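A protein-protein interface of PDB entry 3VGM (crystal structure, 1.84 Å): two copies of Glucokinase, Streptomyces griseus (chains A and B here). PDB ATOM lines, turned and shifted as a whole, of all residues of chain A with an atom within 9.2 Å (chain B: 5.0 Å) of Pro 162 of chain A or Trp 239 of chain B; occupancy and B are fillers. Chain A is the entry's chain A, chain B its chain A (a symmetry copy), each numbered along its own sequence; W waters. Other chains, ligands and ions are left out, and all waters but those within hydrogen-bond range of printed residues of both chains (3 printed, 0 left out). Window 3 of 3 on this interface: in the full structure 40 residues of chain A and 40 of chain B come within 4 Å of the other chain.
Val 160 of chain A touches Pro 162 of chain B, and with the chains exchanged Pro 162 of chain A touches Val 160 of chain B.
Pro 162 of chain B touches its own counterpart, Pro 162 of chain A.
Pro 162 of chain A touches Trp 239 of chain B, and with the chains exchanged Trp 239 of chain A touches Pro 162 of chain B.
6 positions are printed for both chains.
Of the 7 pairs that touch across the chains among the printed residues, 5 have their exchanged pair printed and touching as well.
The backbone NH of Val 160 of chain A lies within hydrogen-bond range of the backbone carbonyl oxygen of Gly 173 of chain A, 2.8 Å away.
O of Trp 239 of chain A lies within hydrogen-bond range of NE1 of Trp 175 of chain A.
The indole nitrogen of Trp 175 of chain B is in hydrogen-bond range of the backbone carbonyl oxygen of Trp 239 of chain B (3.0 Å).
The indole nitrogen (NE1) of Trp 239 of chain B lies close to the side-chain hydroxyl (OH) of Tyr 187 of chain B.
Water W1 lies within hydrogen-bond range of the backbone carbonyl oxygen of Val 160 of chain B (2.8 Å) and the backbone carbonyl oxygen of Arg 159 of chain A (2.8 Å).
Water W3 bridges NH2 of Arg 159 of chain A and O of Arg 238 of chain B.
Water W2 bridges O of Trp 239 of chain B and NH2 of Arg 159 of chain A.
Arg 159 of chain A touches Trp 239 of chain B.
NH2 of Arg 159 of chain A touches CB of Ala 242 of chain B (3.5 Å).
Val 160 of chain A touches Pro 162 of chain B (O to CG, 3.1 Å).
Pro 162 of chain A touches Val 160 of chain B (CG to O, 3.1 Å).
Pro 162 of chain B touches Pro 162 of chain A (CD to CD, 3.8 Å).
CZ3 of Trp 239 of chain B touches CG of Pro 162 of chain A, 3.9 Å away.
Trp 239 of chain A touches Pro 162 of chain B (CZ3 to CG, 3.9 Å).
Of the printed residues of chain B, Pro 162 of chain A touches Val 160 (3.1 Å), Pro 162 (3.8 Å) and Trp 239 (3.9 Å).
Of chain A, only Arg 159 (3.6 Å) and Pro 162 (3.9 Å) come within 4 Å of Trp 239 of chain B.
No residue of chain A comes within 4 Å of Ala 240 of chain B.
Ala 242 of chain B touches just one residue of chain A: Arg 159 (3.5 Å).
Of the printed residues of chain B, Val 160 of chain A touches Pro 162.
Printed residues of chain A within 4 Å of Val 160 of chain B: Pro 162 (3.1 Å).
Printed residues of chain A within 4 Å of Pro 162 of chain B: Val 160 (3.1 Å), Pro 162 (3.8 Å) and Trp 239 (3.9 Å).
Of the printed residues of chain B, Trp 239 of chain A touches Pro 162 (3.9 Å).
Of the printed residues of chain B, Arg 159 of chain A touches Trp 239 and Ala 242.
Arg 238 of chain B touches none of the printed residues of chain A.
Of the 16 printed residues of chain B, 4 touch a printed residue of chain A.
Hydrophobic or aromatic side chains of chain A that line the printed part of chain B: Pro 162 and Trp 239.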
ATOM      1  N   ILE A 158       2.893 -33.513  -4.539  1.00  0.00           N
ATOM      2  CA  ILE A 158       2.665 -32.221  -3.867  1.00  0.00           C
ATOM      3  C   ILE A 158       2.647 -31.116  -4.940  1.00  0.00           C
ATOM      4  O   ILE A 158       3.405 -31.178  -5.923  1.00  0.00           O
ATOM      5  CB  ILE A 158       3.738 -31.918  -2.793  1.00  0.00           C
ATOM      6  CG1 ILE A 158       5.124 -31.816  -3.413  1.00  0.00           C
ATOM      7  CG2 ILE A 158       3.721 -33.001  -1.704  1.00  0.00           C
ATOM      8  CD1 ILE A 158       6.238 -31.331  -2.442  1.00  0.00           C
ATOM      9  N   ARG A 159       1.773 -30.121  -4.763  1.00  0.00           N
ATOM     10  CA  ARG A 159       1.614 -29.082  -5.763  1.00  0.00           C
ATOM     11  C   ARG A 159       2.705 -28.029  -5.594  1.00  0.00           C
ATOM     12  O   ARG A 159       2.713 -27.302  -4.628  1.00  0.00           O
ATOM     13  CB  ARG A 159       0.241 -28.408  -5.646  1.00  0.00           C
ATOM     14  CG  ARG A 159      -0.020 -27.459  -6.826  1.00  0.00           C
ATOM     15  CD  ARG A 159      -1.406 -26.788  -6.714  1.00  0.00           C
ATOM     16  NE  ARG A 159      -1.384 -25.807  -5.638  1.00  0.00           N
ATOM     17  CZ  ARG A 159      -2.396 -24.995  -5.335  1.00  0.00           C
ATOM     18  NH1 ARG A 159      -3.514 -25.017  -6.053  1.00  0.00           N
ATOM     19  NH2 ARG A 159      -2.271 -24.141  -4.331  1.00  0.00           N
ATOM     20  N   VAL A 160       3.602 -27.923  -6.558  1.00  0.00           N
ATOM     21  CA  VAL A 160       4.630 -26.889  -6.491  1.00  0.00           C
ATOM     22  C   VAL A 160       4.299 -25.714  -7.390  1.00  0.00           C
ATOM     23  O   VAL A 160       4.841 -24.622  -7.185  1.00  0.00           O
ATOM     24  CB  VAL A 160       6.062 -27.444  -6.795  1.00  0.00           C
ATOM     25  CG1 VAL A 160       6.447 -28.444  -5.714  1.00  0.00           C
ATOM     26  CG2 VAL A 160       6.185 -28.046  -8.231  1.00  0.00           C
ATOM     27  N   VAL A 161       3.418 -25.915  -8.373  1.00  0.00           N
ATOM     28  CA  VAL A 161       2.972 -24.823  -9.250  1.00  0.00           C
ATOM     29  C   VAL A 161       1.444 -24.765  -9.244  1.00  0.00           C
ATOM     30  O   VAL A 161       0.792 -25.642  -9.834  1.00  0.00           O
ATOM     31  CB  VAL A 161       3.494 -25.000 -10.733  1.00  0.00           C
ATOM     32  CG1 VAL A 161       2.938 -23.889 -11.656  1.00  0.00           C
ATOM     33  CG2 VAL A 161       5.031 -24.990 -10.764  1.00  0.00           C
ATOM     34  N   PRO A 162       0.851 -23.740  -8.589  1.00  0.00           N
ATOM     35  CA  PRO A 162      -0.617 -23.604  -8.652  1.00  0.00           C
ATOM     36  C   PRO A 162      -1.017 -23.440 -10.124  1.00  0.00           C
ATOM     37  O   PRO A 162      -0.335 -22.743 -10.863  1.00  0.00           O
ATOM     38  CB  PRO A 162      -0.912 -22.304  -7.865  1.00  0.00           C
ATOM     39  CG  PRO A 162       0.327 -22.127  -6.945  1.00  0.00           C
ATOM     40  CD  PRO A 162       1.503 -22.685  -7.782  1.00  0.00           C
ATOM     41  N   ASP A 163      -2.094 -24.100 -10.535  1.00  0.00           N
ATOM     42  CA  ASP A 163      -2.546 -24.056 -11.936  1.00  0.00           C
ATOM     43  C   ASP A 163      -1.520 -24.604 -12.926  1.00  0.00           C
ATOM     44  O   ASP A 163      -1.561 -24.271 -14.100  1.00  0.00           O
ATOM     45  CB  ASP A 163      -2.973 -22.630 -12.282  1.00  0.00           C
ATOM     46  CG  ASP A 163      -4.105 -22.145 -11.366  1.00  0.00           C
ATOM     47  OD1 ASP A 163      -5.239 -22.675 -11.512  1.00  0.00           O
ATOM     48  OD2 ASP A 163      -3.839 -21.258 -10.515  1.00  0.00           O
ATOM     49  N   GLY A 164      -0.631 -25.476 -12.453  1.00  0.00           N
ATOM     50  CA  GLY A 164       0.454 -25.995 -13.284  1.00  0.00           C
ATOM     51  C   GLY A 164       0.058 -27.150 -14.201  1.00  0.00           C
ATOM     52  O   GLY A 164      -1.136 -27.411 -14.444  1.00  0.00           O
ATOM     53  N   LEU A 165       1.081 -27.869 -14.657  1.00  0.00           N
ATOM     54  CA  LEU A 165       0.920 -28.953 -15.620  1.00  0.00           C
ATOM     55  C   LEU A 165      -0.010 -30.072 -15.144  1.00  0.00           C
ATOM     56  O   LEU A 165       0.083 -30.521 -13.988  1.00  0.00           O
ATOM     57  CB  LEU A 165       2.306 -29.554 -15.946  1.00  0.00           C
ATOM     58  CG  LEU A 165       3.196 -28.651 -16.801  1.00  0.00           C
ATOM     59  CD1 LEU A 165       4.643 -29.210 -16.742  1.00  0.00           C
ATOM     60  CD2 LEU A 165       2.691 -28.703 -18.273  1.00  0.00           C
ATOM     61  N   SER A 171      -4.224 -34.634 -11.045  1.00  0.00           N
ATOM     62  CA  SER A 171      -4.199 -33.267 -10.524  1.00  0.00           C
ATOM     63  C   SER A 171      -3.337 -32.357 -11.413  1.00  0.00           C
ATOM     64  O   SER A 171      -3.025 -32.722 -12.566  1.00  0.00           O
ATOM     65  CB  SER A 171      -3.673 -33.244  -9.071  1.00  0.00           C
ATOM     66  OG  SER A 171      -4.057 -32.024  -8.444  1.00  0.00           O
ATOM     67  N   GLN A 172      -2.973 -31.186 -10.876  1.00  0.00           N
ATOM     68  CA  GLN A 172      -2.160 -30.195 -11.580  1.00  0.00           C
ATOM     69  C   GLN A 172      -1.009 -29.711 -10.742  1.00  0.00           C
ATOM     70  O   GLN A 172      -1.156 -29.522  -9.525  1.00  0.00           O
ATOM     71  CB  GLN A 172      -2.977 -28.929 -11.866  1.00  0.00           C
ATOM     72  CG  GLN A 172      -3.790 -29.008 -13.137  1.00  0.00           C
ATOM     73  CD  GLN A 172      -4.560 -27.709 -13.355  1.00  0.00           C
ATOM     74  OE1 GLN A 172      -5.764 -27.663 -13.097  1.00  0.00           O
ATOM     75  NE2 GLN A 172      -3.876 -26.652 -13.808  1.00  0.00           N
ATOM     76  N   GLY A 173       0.101 -29.428 -11.414  1.00  0.00           N
ATOM     77  CA  GLY A 173       1.208 -28.658 -10.794  1.00  0.00           C
ATOM     78  C   GLY A 173       2.094 -29.479  -9.891  1.00  0.00           C
ATOM     79  O   GLY A 173       2.853 -28.909  -9.107  1.00  0.00           O
ATOM     80  N   CYS A 174       1.979 -30.813  -9.980  1.00  0.00           N
ATOM     81  CA  CYS A 174       2.770 -31.748  -9.154  1.00  0.00           C
ATOM     82  C   CYS A 174       4.287 -31.634  -9.337  1.00  0.00           C
ATOM     83  O   CYS A 174       4.797 -31.437 -10.459  1.00  0.00           O
ATOM     84  CB  CYS A 174       2.345 -33.192  -9.490  1.00  0.00           C
ATOM     85  SG  CYS A 174       0.602 -33.446  -9.090  1.00  0.00           S
ATOM     86  N   TRP A 175       5.016 -31.836  -8.238  1.00  0.00           N
ATOM     87  CA  TRP A 175       6.491 -31.782  -8.251  1.00  0.00           C
ATOM     88  C   TRP A 175       7.066 -32.711  -9.334  1.00  0.00           C
ATOM     89  O   TRP A 175       8.023 -32.365 -10.005  1.00  0.00           O
ATOM     90  CB  TRP A 175       7.015 -32.189  -6.872  1.00  0.00           C
ATOM     91  CG  TRP A 175       8.449 -31.853  -6.607  1.00  0.00           C
ATOM     92  CD1 TRP A 175       9.237 -30.933  -7.257  1.00  0.00           C
ATOM     93  CD2 TRP A 175       9.255 -32.427  -5.581  1.00  0.00           C
ATOM     94  NE1 TRP A 175      10.509 -30.920  -6.704  1.00  0.00           N
ATOM     95  CE2 TRP A 175      10.537 -31.832  -5.673  1.00  0.00           C
ATOM     96  CE3 TRP A 175       9.006 -33.386  -4.567  1.00  0.00           C
ATOM     97  CZ2 TRP A 175      11.577 -32.159  -4.803  1.00  0.00           C
ATOM     98  CZ3 TRP A 175      10.059 -33.736  -3.710  1.00  0.00           C
ATOM     99  CH2 TRP A 175      11.322 -33.091  -3.816  1.00  0.00           C
ATOM    100  N   TYR A 178       7.909 -31.393 -12.753  1.00  0.00           N
ATOM    101  CA  TYR A 178       8.998 -30.415 -12.836  1.00  0.00           C
ATOM    102  C   TYR A 178      10.370 -30.973 -12.450  1.00  0.00           C
ATOM    103  O   TYR A 178      11.393 -30.379 -12.801  1.00  0.00           O
ATOM    104  CB  TYR A 178       8.675 -29.182 -11.940  1.00  0.00           C
ATOM    105  CG  TYR A 178       7.396 -28.551 -12.375  1.00  0.00           C
ATOM    106  CD1 TYR A 178       6.213 -28.840 -11.694  1.00  0.00           C
ATOM    107  CD2 TYR A 178       7.340 -27.763 -13.541  1.00  0.00           C
ATOM    108  CE1 TYR A 178       5.015 -28.325 -12.110  1.00  0.00           C
ATOM    109  CE2 TYR A 178       6.117 -27.249 -13.984  1.00  0.00           C
ATOM    110  CZ  TYR A 178       4.967 -27.533 -13.255  1.00  0.00           C
ATOM    111  OH  TYR A 178       3.739 -27.017 -13.690  1.00  0.00           O
ATOM    112  N   TRP A 239      14.108 -27.002  -9.412  1.00  0.00           N
ATOM    113  CA  TRP A 239      12.860 -27.564  -8.865  1.00  0.00           C
ATOM    114  C   TRP A 239      13.156 -28.605  -7.802  1.00  0.00           C
ATOM    115  O   TRP A 239      12.475 -28.638  -6.777  1.00  0.00           O
ATOM    116  CB  TRP A 239      11.996 -28.189  -9.981  1.00  0.00           C
ATOM    117  CG  TRP A 239      11.426 -27.128 -10.916  1.00  0.00           C
ATOM    118  CD1 TRP A 239      11.859 -26.834 -12.179  1.00  0.00           C
ATOM    119  CD2 TRP A 239      10.370 -26.202 -10.628  1.00  0.00           C
ATOM    120  NE1 TRP A 239      11.116 -25.799 -12.707  1.00  0.00           N
ATOM    121  CE2 TRP A 239      10.192 -25.398 -11.779  1.00  0.00           C
ATOM    122  CE3 TRP A 239       9.528 -25.992  -9.520  1.00  0.00           C
ATOM    123  CZ2 TRP A 239       9.217 -24.377 -11.861  1.00  0.00           C
ATOM    124  CZ3 TRP A 239       8.516 -24.960  -9.613  1.00  0.00           C
ATOM    125  CH2 TRP A 239       8.398 -24.171 -10.767  1.00  0.00           C
ATOM    126  N   VAL B 160       4.324 -22.339  -1.698  1.00  0.00           N
ATOM    127  CA  VAL B 160       3.158 -22.729  -2.483  1.00  0.00           C
ATOM    128  C   VAL B 160       3.067 -21.942  -3.775  1.00  0.00           C
ATOM    129  O   VAL B 160       2.386 -22.383  -4.708  1.00  0.00           O
ATOM    130  CB  VAL B 160       1.825 -22.630  -1.670  1.00  0.00           C
ATOM    131  CG1 VAL B 160       1.869 -23.627  -0.520  1.00  0.00           C
ATOM    132  CG2 VAL B 160       1.518 -21.178  -1.184  1.00  0.00           C
ATOM    133  N   VAL B 161       3.745 -20.794  -3.850  1.00  0.00           N
ATOM    134  CA  VAL B 161       3.785 -19.996  -5.083  1.00  0.00           C
ATOM    135  C   VAL B 161       5.242 -19.723  -5.460  1.00  0.00           C
ATOM    136  O   VAL B 161       5.909 -18.914  -4.793  1.00  0.00           O
ATOM    137  CB  VAL B 161       3.007 -18.627  -4.932  1.00  0.00           C
ATOM    138  CG1 VAL B 161       3.140 -17.766  -6.211  1.00  0.00           C
ATOM    139  CG2 VAL B 161       1.524 -18.885  -4.623  1.00  0.00           C
ATOM    140  N   PRO B 162       5.756 -20.380  -6.525  1.00  0.00           N
ATOM    141  CA  PRO B 162       7.127 -20.061  -6.969  1.00  0.00           C
ATOM    142  C   PRO B 162       7.172 -18.574  -7.342  1.00  0.00           C
ATOM    143  O   PRO B 162       6.232 -18.071  -7.943  1.00  0.00           O
ATOM    144  CB  PRO B 162       7.330 -20.939  -8.229  1.00  0.00           C
ATOM    145  CG  PRO B 162       6.301 -22.090  -8.061  1.00  0.00           C
ATOM    146  CD  PRO B 162       5.102 -21.424  -7.345  1.00  0.00           C
ATOM    147  N   TRP B 175       3.349 -20.467   2.263  1.00  0.00           N
ATOM    148  CA  TRP B 175       1.921 -20.738   2.517  1.00  0.00           C
ATOM    149  C   TRP B 175       1.317 -19.672   3.448  1.00  0.00           C
ATOM    150  O   TRP B 175       0.193 -19.242   3.252  1.00  0.00           O
ATOM    151  CB  TRP B 175       1.783 -22.127   3.145  1.00  0.00           C
ATOM    152  CG  TRP B 175       0.399 -22.697   3.141  1.00  0.00           C
ATOM    153  CD1 TRP B 175      -0.666 -22.330   2.352  1.00  0.00           C
ATOM    154  CD2 TRP B 175      -0.053 -23.774   3.958  1.00  0.00           C
ATOM    155  NE1 TRP B 175      -1.773 -23.108   2.655  1.00  0.00           N
ATOM    156  CE2 TRP B 175      -1.414 -24.001   3.639  1.00  0.00           C
ATOM    157  CE3 TRP B 175       0.578 -24.592   4.929  1.00  0.00           C
ATOM    158  CZ2 TRP B 175      -2.168 -25.001   4.252  1.00  0.00           C
ATOM    159  CZ3 TRP B 175      -0.187 -25.580   5.566  1.00  0.00           C
ATOM    160  CH2 TRP B 175      -1.543 -25.795   5.192  1.00  0.00           C
ATOM    161  N   TYR B 178      -0.455 -16.670   2.041  1.00  0.00           N
ATOM    162  CA  TYR B 178      -1.701 -16.917   1.309  1.00  0.00           C
ATOM    163  C   TYR B 178      -2.832 -17.479   2.173  1.00  0.00           C
ATOM    164  O   TYR B 178      -3.999 -17.404   1.778  1.00  0.00           O
ATOM    165  CB  TYR B 178      -1.435 -17.887   0.119  1.00  0.00           C
ATOM    166  CG  TYR B 178      -0.416 -17.305  -0.801  1.00  0.00           C
ATOM    167  CD1 TYR B 178       0.916 -17.709  -0.708  1.00  0.00           C
ATOM    168  CD2 TYR B 178      -0.754 -16.259  -1.683  1.00  0.00           C
ATOM    169  CE1 TYR B 178       1.882 -17.146  -1.496  1.00  0.00           C
ATOM    170  CE2 TYR B 178       0.230 -15.664  -2.478  1.00  0.00           C
ATOM    171  CZ  TYR B 178       1.540 -16.123  -2.378  1.00  0.00           C
ATOM    172  OH  TYR B 178       2.531 -15.535  -3.175  1.00  0.00           O
ATOM    173  N   ALA B 179      -2.508 -18.062   3.334  1.00  0.00           N
ATOM    174  CA  ALA B 179      -3.554 -18.755   4.115  1.00  0.00           C
ATOM    175  C   ALA B 179      -3.646 -18.291   5.577  1.00  0.00           C
ATOM    176  O   ALA B 179      -4.378 -18.868   6.373  1.00  0.00           O
ATOM    177  CB  ALA B 179      -3.391 -20.320   4.004  1.00  0.00           C
ATOM    178  N   TYR B 187      -6.698  -9.953   0.869  1.00  0.00           N
ATOM    179  CA  TYR B 187      -7.782 -10.249  -0.079  1.00  0.00           C
ATOM    180  C   TYR B 187      -8.937  -9.267   0.084  1.00  0.00           C
ATOM    181  O   TYR B 187      -9.487  -8.783  -0.900  1.00  0.00           O
ATOM    182  CB  TYR B 187      -8.305 -11.686   0.102  1.00  0.00           C
ATOM    183  CG  TYR B 187      -7.220 -12.753  -0.010  1.00  0.00           C
ATOM    184  CD1 TYR B 187      -6.203 -12.648  -0.979  1.00  0.00           C
ATOM    185  CD2 TYR B 187      -7.232 -13.868   0.835  1.00  0.00           C
ATOM    186  CE1 TYR B 187      -5.198 -13.629  -1.072  1.00  0.00           C
ATOM    187  CE2 TYR B 187      -6.230 -14.867   0.737  1.00  0.00           C
ATOM    188  CZ  TYR B 187      -5.222 -14.712  -0.229  1.00  0.00           C
ATOM    189  OH  TYR B 187      -4.224 -15.641  -0.329  1.00  0.00           O
ATOM    190  N   GLU B 235     -11.370 -17.151  -0.762  1.00  0.00           N
ATOM    191  CA  GLU B 235     -10.052 -17.098  -1.356  1.00  0.00           C
ATOM    192  C   GLU B 235      -9.006 -17.729  -0.429  1.00  0.00           C
ATOM    193  O   GLU B 235      -8.166 -18.544  -0.872  1.00  0.00           O
ATOM    194  CB  GLU B 235      -9.699 -15.638  -1.695  1.00  0.00           C
ATOM    195  CG  GLU B 235      -8.370 -15.496  -2.428  1.00  0.00           C
ATOM    196  CD  GLU B 235      -8.287 -14.185  -3.238  1.00  0.00           C
ATOM    197  OE1 GLU B 235      -9.246 -13.368  -3.228  1.00  0.00           O
ATOM    198  OE2 GLU B 235      -7.255 -13.987  -3.893  1.00  0.00           O
ATOM    199  N   LEU B 236      -9.070 -17.392   0.859  1.00  0.00           N
ATOM    200  CA  LEU B 236      -8.139 -17.978   1.853  1.00  0.00           C
ATOM    201  C   LEU B 236      -8.352 -19.502   1.905  1.00  0.00           C
ATOM    202  O   LEU B 236      -7.386 -20.289   1.935  1.00  0.00           O
ATOM    203  CB  LEU B 236      -8.355 -17.349   3.249  1.00  0.00           C
ATOM    204  CG  LEU B 236      -7.452 -17.901   4.365  1.00  0.00           C
ATOM    205  CD1 LEU B 236      -7.086 -16.835   5.365  1.00  0.00           C
ATOM    206  CD2 LEU B 236      -8.098 -19.114   5.083  1.00  0.00           C
ATOM    207  N   ALA B 237      -9.617 -19.914   1.867  1.00  0.00           N
ATOM    208  CA  ALA B 237      -9.958 -21.342   1.996  1.00  0.00           C
ATOM    209  C   ALA B 237      -9.398 -22.179   0.869  1.00  0.00           C
ATOM    210  O   ALA B 237      -9.047 -23.349   1.079  1.00  0.00           O
ATOM    211  CB  ALA B 237     -11.495 -21.540   2.099  1.00  0.00           C
ATOM    212  N   ARG B 238      -9.315 -21.602  -0.330  1.00  0.00           N
ATOM    213  CA  ARG B 238      -8.730 -22.320  -1.451  1.00  0.00           C
ATOM    214  C   ARG B 238      -7.261 -22.627  -1.174  1.00  0.00           C
ATOM    215  O   ARG B 238      -6.811 -23.746  -1.426  1.00  0.00           O
ATOM    216  CB  ARG B 238      -8.872 -21.536  -2.762  1.00  0.00           C
ATOM    217  CG  ARG B 238     -10.327 -21.585  -3.304  1.00  0.00           C
ATOM    218  CD  ARG B 238     -10.412 -21.025  -4.718  1.00  0.00           C
ATOM    219  NE  ARG B 238     -10.271 -19.559  -4.776  1.00  0.00           N
ATOM    220  CZ  ARG B 238     -11.280 -18.702  -4.592  1.00  0.00           C
ATOM    221  NH1 ARG B 238     -12.504 -19.148  -4.302  1.00  0.00           N
ATOM    222  NH2 ARG B 238     -11.066 -17.401  -4.694  1.00  0.00           N
ATOM    223  N   TRP B 239      -6.528 -21.645  -0.646  1.00  0.00           N
ATOM    224  CA  TRP B 239      -5.111 -21.872  -0.312  1.00  0.00           C
ATOM    225  C   TRP B 239      -4.978 -22.830   0.857  1.00  0.00           C
ATOM    226  O   TRP B 239      -4.103 -23.697   0.837  1.00  0.00           O
ATOM    227  CB  TRP B 239      -4.398 -20.545   0.018  1.00  0.00           C
ATOM    228  CG  TRP B 239      -4.245 -19.662  -1.217  1.00  0.00           C
ATOM    229  CD1 TRP B 239      -4.980 -18.551  -1.522  1.00  0.00           C
ATOM    230  CD2 TRP B 239      -3.345 -19.864  -2.314  1.00  0.00           C
ATOM    231  NE1 TRP B 239      -4.571 -18.030  -2.732  1.00  0.00           N
ATOM    232  CE2 TRP B 239      -3.566 -18.812  -3.235  1.00  0.00           C
ATOM    233  CE3 TRP B 239      -2.345 -20.812  -2.597  1.00  0.00           C
ATOM    234  CZ2 TRP B 239      -2.838 -18.679  -4.441  1.00  0.00           C
ATOM    235  CZ3 TRP B 239      -1.586 -20.663  -3.822  1.00  0.00           C
ATOM    236  CH2 TRP B 239      -1.862 -19.618  -4.716  1.00  0.00           C
ATOM    237  N   ALA B 240      -5.814 -22.661   1.886  1.00  0.00           N
ATOM    238  CA  ALA B 240      -5.714 -23.516   3.059  1.00  0.00           C
ATOM    239  C   ALA B 240      -6.039 -24.981   2.692  1.00  0.00           C
ATOM    240  O   ALA B 240      -5.332 -25.895   3.102  1.00  0.00           O
ATOM    241  CB  ALA B 240      -6.679 -23.019   4.162  1.00  0.00           C
ATOM    242  N   GLY B 241      -7.107 -25.188   1.917  1.00  0.00           N
ATOM    243  CA  GLY B 241      -7.512 -26.557   1.518  1.00  0.00           C
ATOM    244  C   GLY B 241      -6.499 -27.216   0.588  1.00  0.00           C
ATOM    245  O   GLY B 241      -6.224 -28.417   0.698  1.00  0.00           O
ATOM    246  N   ALA B 242      -5.959 -26.448  -0.359  1.00  0.00           N
ATOM    247  CA  ALA B 242      -4.932 -26.998  -1.273  1.00  0.00           C
ATOM    248  C   ALA B 242      -3.685 -27.428  -0.474  1.00  0.00           C
ATOM    249  O   ALA B 242      -3.055 -28.474  -0.753  1.00  0.00           O
ATOM    250  CB  ALA B 242      -4.534 -25.945  -2.337  1.00  0.00           C
ATOM    251  N   GLY B 243      -3.290 -26.594   0.483  1.00  0.00           N
ATOM    252  CA  GLY B 243      -2.159 -26.937   1.351  1.00  0.00           C
ATOM    253  C   GLY B 243      -2.427 -28.183   2.186  1.00  0.00           C
ATOM    254  O   GLY B 243      -1.526 -29.019   2.349  1.00  0.00           O
HETATM  255  O   HOH W   1       1.234 -24.881  -4.544  1.00  0.00           O
HETATM  256  O   HOH W   2      -1.673 -23.725  -0.999  1.00  0.00           O
HETATM  257  O   HOH W   3      -5.006 -22.975  -4.115  1.00  0.00           O
